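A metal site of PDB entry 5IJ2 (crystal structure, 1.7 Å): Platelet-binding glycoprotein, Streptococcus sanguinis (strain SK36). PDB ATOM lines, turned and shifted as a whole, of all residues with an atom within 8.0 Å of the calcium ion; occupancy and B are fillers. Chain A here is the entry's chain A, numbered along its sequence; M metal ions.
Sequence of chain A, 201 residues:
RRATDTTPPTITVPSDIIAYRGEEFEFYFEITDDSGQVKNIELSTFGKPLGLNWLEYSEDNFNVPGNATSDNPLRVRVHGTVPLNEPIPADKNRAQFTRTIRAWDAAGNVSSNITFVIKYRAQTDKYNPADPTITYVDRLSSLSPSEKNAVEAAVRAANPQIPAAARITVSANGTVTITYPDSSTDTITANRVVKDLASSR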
ATOM      1  N   THR A   4      -2.351   0.353  11.445  1.00  0.00           N
ATOM      2  CA  THR A   4      -1.114  -0.226  11.946  1.00  0.00           C
ATOM      3  C   THR A   4       0.023   0.772  11.776  1.00  0.00           C
ATOM      4  O   THR A   4      -0.016   1.672  10.935  1.00  0.00           O
ATOM      5  CB  THR A   4      -0.735  -1.514  11.203  1.00  0.00           C
ATOM      6  OG1 THR A   4      -0.723  -1.264   9.797  1.00  0.00           O
ATOM      7  CG2 THR A   4      -1.718  -2.642  11.494  1.00  0.00           C
ATOM      8  N   ASP A   5       1.040   0.579  12.606  1.00  0.00           N
ATOM      9  CA  ASP A   5       2.295   1.311  12.562  1.00  0.00           C
ATOM     10  C   ASP A   5       3.221   0.623  11.558  1.00  0.00           C
ATOM     11  O   ASP A   5       3.623  -0.528  11.761  1.00  0.00           O
ATOM     12  CB  ASP A   5       2.896   1.334  13.967  1.00  0.00           C
ATOM     13  CG  ASP A   5       4.167   2.158  14.063  1.00  0.00           C
ATOM     14  OD1 ASP A   5       4.755   2.479  13.018  1.00  0.00           O
ATOM     15  OD2 ASP A   5       4.614   2.470  15.196  1.00  0.00           O
ATOM     16  N   THR A   6       3.571   1.324  10.499  1.00  0.00           N
ATOM     17  CA  THR A   6       4.436   0.766   9.473  1.00  0.00           C
ATOM     18  C   THR A   6       5.668   1.625   9.283  1.00  0.00           C
ATOM     19  O   THR A   6       6.406   1.441   8.313  1.00  0.00           O
ATOM     20  CB  THR A   6       3.701   0.631   8.142  1.00  0.00           C
ATOM     21  OG1 THR A   6       3.322   1.933   7.703  1.00  0.00           O
ATOM     22  CG2 THR A   6       2.433  -0.237   8.277  1.00  0.00           C
ATOM     23  N   THR A   7       5.919   2.540  10.216  1.00  0.00           N
ATOM     24  CA  THR A   7       6.947   3.559  10.060  1.00  0.00           C
ATOM     25  C   THR A   7       8.009   3.353  11.114  1.00  0.00           C
ATOM     26  O   THR A   7       7.664   3.375  12.313  1.00  0.00           O
ATOM     27  CB  THR A   7       6.334   4.943  10.215  1.00  0.00           C
ATOM     28  OG1 THR A   7       5.273   5.082   9.266  1.00  0.00           O
ATOM     29  CG2 THR A   7       7.409   6.034   9.958  1.00  0.00           C
ATOM     30  N   PRO A   8       9.280   3.185  10.768  1.00  0.00           N
ATOM     31  CA  PRO A   8      10.288   2.949  11.786  1.00  0.00           C
ATOM     32  C   PRO A   8      10.636   4.228  12.505  1.00  0.00           C
ATOM     33  O   PRO A   8      10.275   5.340  12.071  1.00  0.00           O
ATOM     34  CB  PRO A   8      11.494   2.420  10.983  1.00  0.00           C
ATOM     35  CG  PRO A   8      11.270   2.879   9.602  1.00  0.00           C
ATOM     36  CD  PRO A   8       9.803   3.056   9.390  1.00  0.00           C
ATOM     37  N   PRO A   9      11.371   4.100  13.604  1.00  0.00           N
ATOM     38  CA  PRO A   9      11.839   5.269  14.347  1.00  0.00           C
ATOM     39  C   PRO A   9      12.768   6.109  13.500  1.00  0.00           C
ATOM     40  O   PRO A   9      13.314   5.669  12.488  1.00  0.00           O
ATOM     41  CB  PRO A   9      12.592   4.664  15.540  1.00  0.00           C
ATOM     42  CG  PRO A   9      11.987   3.286  15.695  1.00  0.00           C
ATOM     43  CD  PRO A   9      11.670   2.833  14.290  1.00  0.00           C
ATOM     44  N   THR A  10      12.954   7.344  13.957  1.00  0.00           N
ATOM     45  CA  THR A  10      13.845   8.309  13.333  1.00  0.00           C
ATOM     46  C   THR A  10      14.942   8.658  14.320  1.00  0.00           C
ATOM     47  O   THR A  10      14.658   9.032  15.473  1.00  0.00           O
ATOM     48  CB  THR A  10      13.073   9.589  12.950  1.00  0.00           C
ATOM     49  OG1 THR A  10      12.086   9.282  11.960  1.00  0.00           O
ATOM     50  CG2 THR A  10      14.018  10.602  12.394  1.00  0.00           C
ATOM     51  N   THR A  32      12.953   9.292  17.971  1.00  0.00           N
ATOM     52  CA  THR A  32      11.515   9.460  18.077  1.00  0.00           C
ATOM     53  C   THR A  32      10.840   8.377  17.236  1.00  0.00           C
ATOM     54  O   THR A  32      11.454   7.806  16.334  1.00  0.00           O
ATOM     55  CB  THR A  32      11.027  10.821  17.586  1.00  0.00           C
ATOM     56  OG1 THR A  32      11.219  10.882  16.167  1.00  0.00           O
ATOM     57  CG2 THR A  32      11.764  11.965  18.270  1.00  0.00           C
ATOM     58  N   ASP A  33       9.597   8.073  17.554  1.00  0.00           N
ATOM     59  CA  ASP A  33       8.811   7.185  16.701  1.00  0.00           C
ATOM     60  C   ASP A  33       7.392   7.728  16.658  1.00  0.00           C
ATOM     61  O   ASP A  33       6.907   8.293  17.631  1.00  0.00           O
ATOM     62  CB  ASP A  33       8.796   5.752  17.211  1.00  0.00           C
ATOM     63  CG  ASP A  33       8.093   4.815  16.237  1.00  0.00           C
ATOM     64  OD1 ASP A  33       8.643   4.597  15.148  1.00  0.00           O
ATOM     65  OD2 ASP A  33       6.976   4.307  16.524  1.00  0.00           O
ATOM     66  N   ASP A  34       6.716   7.511  15.514  1.00  0.00           N
ATOM     67  CA  ASP A  34       5.352   8.010  15.399  1.00  0.00           C
ATOM     68  C   ASP A  34       4.423   7.431  16.464  1.00  0.00           C
ATOM     69  O   ASP A  34       3.448   8.079  16.843  1.00  0.00           O
ATOM     70  CB  ASP A  34       4.820   7.767  13.975  1.00  0.00           C
ATOM     71  CG  ASP A  34       4.727   6.274  13.599  1.00  0.00           C
ATOM     72  OD1 ASP A  34       5.575   5.450  14.003  1.00  0.00           O
ATOM     73  OD2 ASP A  34       3.796   5.933  12.829  1.00  0.00           O
ATOM     74  N   SER A  35       4.719   6.230  16.966  1.00  0.00           N
ATOM     75  CA  SER A  35       3.951   5.609  18.049  1.00  0.00           C
ATOM     76  C   SER A  35       4.265   6.193  19.401  1.00  0.00           C
ATOM     77  O   SER A  35       3.543   5.908  20.378  1.00  0.00           O
ATOM     78  CB  SER A  35       4.249   4.119  18.137  1.00  0.00           C
ATOM     79  OG  SER A  35       5.564   3.875  18.638  1.00  0.00           O
ATOM     80  N   GLY A  36       5.367   6.922  19.526  1.00  0.00           N
ATOM     81  CA  GLY A  36       5.837   7.350  20.817  1.00  0.00           C
ATOM     82  C   GLY A  36       6.687   6.344  21.585  1.00  0.00           C
ATOM     83  O   GLY A  36       7.111   6.669  22.701  1.00  0.00           O
ATOM     84  N   GLN A  37       6.963   5.161  21.042  1.00  0.00           N
ATOM     85  CA  GLN A  37       7.696   4.134  21.774  1.00  0.00           C
ATOM     86  C   GLN A  37       8.807   3.528  20.923  1.00  0.00           C
ATOM     87  O   GLN A  37       8.546   3.042  19.818  1.00  0.00           O
ATOM     88  CB  GLN A  37       6.763   3.003  22.236  1.00  0.00           C
ATOM     89  CG  GLN A  37       7.467   1.912  23.046  1.00  0.00           C
ATOM     90  CD  GLN A  37       6.485   0.971  23.697  1.00  0.00           C
ATOM     91  OE1 GLN A  37       5.288   1.272  23.787  1.00  0.00           O
ATOM     92  NE2 GLN A  37       6.971  -0.200  24.117  1.00  0.00           N
ATOM     93  N   VAL A  38      10.031   3.537  21.459  1.00  0.00           N
ATOM     94  CA  VAL A  38      11.168   2.894  20.837  1.00  0.00           C
ATOM     95  C   VAL A  38      11.560   1.712  21.722  1.00  0.00           C
ATOM     96  O   VAL A  38      11.721   1.876  22.939  1.00  0.00           O
ATOM     97  CB  VAL A  38      12.339   3.870  20.620  1.00  0.00           C
ATOM     98  CG1 VAL A  38      13.678   3.098  20.427  1.00  0.00           C
ATOM     99  CG2 VAL A  38      12.007   4.722  19.392  1.00  0.00           C
ATOM    100  N   TRP A 104      14.431  -0.074  16.621  1.00  0.00           N
ATOM    101  CA  TRP A 104      13.129  -0.688  16.443  1.00  0.00           C
ATOM    102  C   TRP A 104      12.067   0.083  17.227  1.00  0.00           C
ATOM    103  O   TRP A 104      12.333   0.552  18.334  1.00  0.00           O
ATOM    104  CB  TRP A 104      13.131  -2.130  16.976  1.00  0.00           C
ATOM    105  CG  TRP A 104      13.828  -3.137  16.173  1.00  0.00           C
ATOM    106  CD1 TRP A 104      13.239  -4.092  15.408  1.00  0.00           C
ATOM    107  CD2 TRP A 104      15.241  -3.380  16.111  1.00  0.00           C
ATOM    108  NE1 TRP A 104      14.188  -4.889  14.833  1.00  0.00           N
ATOM    109  CE2 TRP A 104      15.432  -4.486  15.253  1.00  0.00           C
ATOM    110  CE3 TRP A 104      16.361  -2.772  16.704  1.00  0.00           C
ATOM    111  CZ2 TRP A 104      16.689  -4.982  14.924  1.00  0.00           C
ATOM    112  CZ3 TRP A 104      17.624  -3.268  16.397  1.00  0.00           C
ATOM    113  CH2 TRP A 104      17.780  -4.365  15.517  1.00  0.00           C
ATOM    114  N   ASP A 105      10.863   0.159  16.682  1.00  0.00           N
ATOM    115  CA  ASP A 105       9.717   0.544  17.502  1.00  0.00           C
ATOM    116  C   ASP A 105       9.089  -0.727  18.098  1.00  0.00           C
ATOM    117  O   ASP A 105       9.636  -1.823  17.985  1.00  0.00           O
ATOM    118  CB  ASP A 105       8.735   1.402  16.700  1.00  0.00           C
ATOM    119  CG  ASP A 105       8.068   0.655  15.545  1.00  0.00           C
ATOM    120  OD1 ASP A 105       8.127  -0.593  15.501  1.00  0.00           O
ATOM    121  OD2 ASP A 105       7.491   1.331  14.665  1.00  0.00           O
ATOM    122  N   ALA A 106       7.927  -0.591  18.757  1.00  0.00           N
ATOM    123  CA  ALA A 106       7.280  -1.742  19.374  1.00  0.00           C
ATOM    124  C   ALA A 106       6.385  -2.519  18.410  1.00  0.00           C
ATOM    125  O   ALA A 106       5.660  -3.417  18.853  1.00  0.00           O
ATOM    126  CB  ALA A 106       6.438  -1.305  20.573  1.00  0.00           C
ATOM    127  N   ALA A 107       6.392  -2.173  17.138  1.00  0.00           N
ATOM    128  CA  ALA A 107       5.552  -2.831  16.151  1.00  0.00           C
ATOM    129  C   ALA A 107       6.396  -3.574  15.138  1.00  0.00           C
ATOM    130  O   ALA A 107       5.879  -3.956  14.085  1.00  0.00           O
ATOM    131  CB  ALA A 107       4.652  -1.811  15.453  1.00  0.00           C
ATOM    132  N   GLY A 108       7.685  -3.732  15.401  1.00  0.00           N
ATOM    133  CA  GLY A 108       8.561  -4.471  14.523  1.00  0.00           C
ATOM    134  C   GLY A 108       9.229  -3.679  13.410  1.00  0.00           C
ATOM    135  O   GLY A 108       9.966  -4.270  12.616  1.00  0.00           O
ATOM    136  N   ASN A 109       8.966  -2.385  13.300  1.00  0.00           N
ATOM    137  CA  ASN A 109       9.631  -1.583  12.287  1.00  0.00           C
ATOM    138  C   ASN A 109      11.014  -1.197  12.764  1.00  0.00           C
ATOM    139  O   ASN A 109      11.167  -0.599  13.836  1.00  0.00           O
ATOM    140  CB  ASN A 109       8.802  -0.345  11.986  1.00  0.00           C
ATOM    141  CG  ASN A 109       7.371  -0.682  11.630  1.00  0.00           C
ATOM    142  OD1 ASN A 109       7.126  -1.315  10.603  1.00  0.00           O
ATOM    143  ND2 ASN A 109       6.428  -0.291  12.481  1.00  0.00           N
ATOM    144  N   VAL A 110      12.035  -1.497  11.966  1.00  0.00           N
ATOM    145  CA  VAL A 110      13.409  -1.134  12.296  1.00  0.00           C
ATOM    146  C   VAL A 110      13.883  -0.113  11.276  1.00  0.00           C
ATOM    147  O   VAL A 110      13.585  -0.220  10.080  1.00  0.00           O
ATOM    148  CB  VAL A 110      14.337  -2.367  12.364  1.00  0.00           C
ATOM    149  CG1 VAL A 110      14.335  -3.182  11.040  1.00  0.00           C
ATOM    150  CG2 VAL A 110      15.737  -1.947  12.762  1.00  0.00           C
HETATM  151 CA    CA M   1       6.609   3.472  14.299  1.00  0.00          CA
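The backbone NH of Asn 109 sits at hydrogen-bond distance from the side-chain carboxylate of Asp 105, 3.0 Å away.
OD1 of Asp 105 sits at hydrogen-bond distance from N of Ala 107.
OD1 of Asp 105 is in hydrogen-bond range of N of Gly 108, at 3.2 Å.
OG of Ser 35 lies close to OD2 of Asp 33.
The side-chain amide nitrogen (ND2) of Asn 109 sits at hydrogen-bond distance from the backbone carbonyl oxygen (O) of Asp 5 (2.9 Å).
Five residues have an atom within 4 Å of the calcium ion: Asp 5, Thr 7, Asp 33, Asp 34 and Asp 105.
The nearest printed residue that does not touch the calcium ion is Asn 109 (4.2 Å).
The calcium ion is bound by O of Thr 7 (2.3 Å), OD1 of Asp 34 (2.3 Å), OD2 of Asp 105 (2.3 Å), OD2 of Asp 33 (2.4 Å), OD2 of Asp 5 (2.4 Å), OD1 of Asp 5 (2.5 Å) and OD1 of Asp 33 (2.5 Å).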
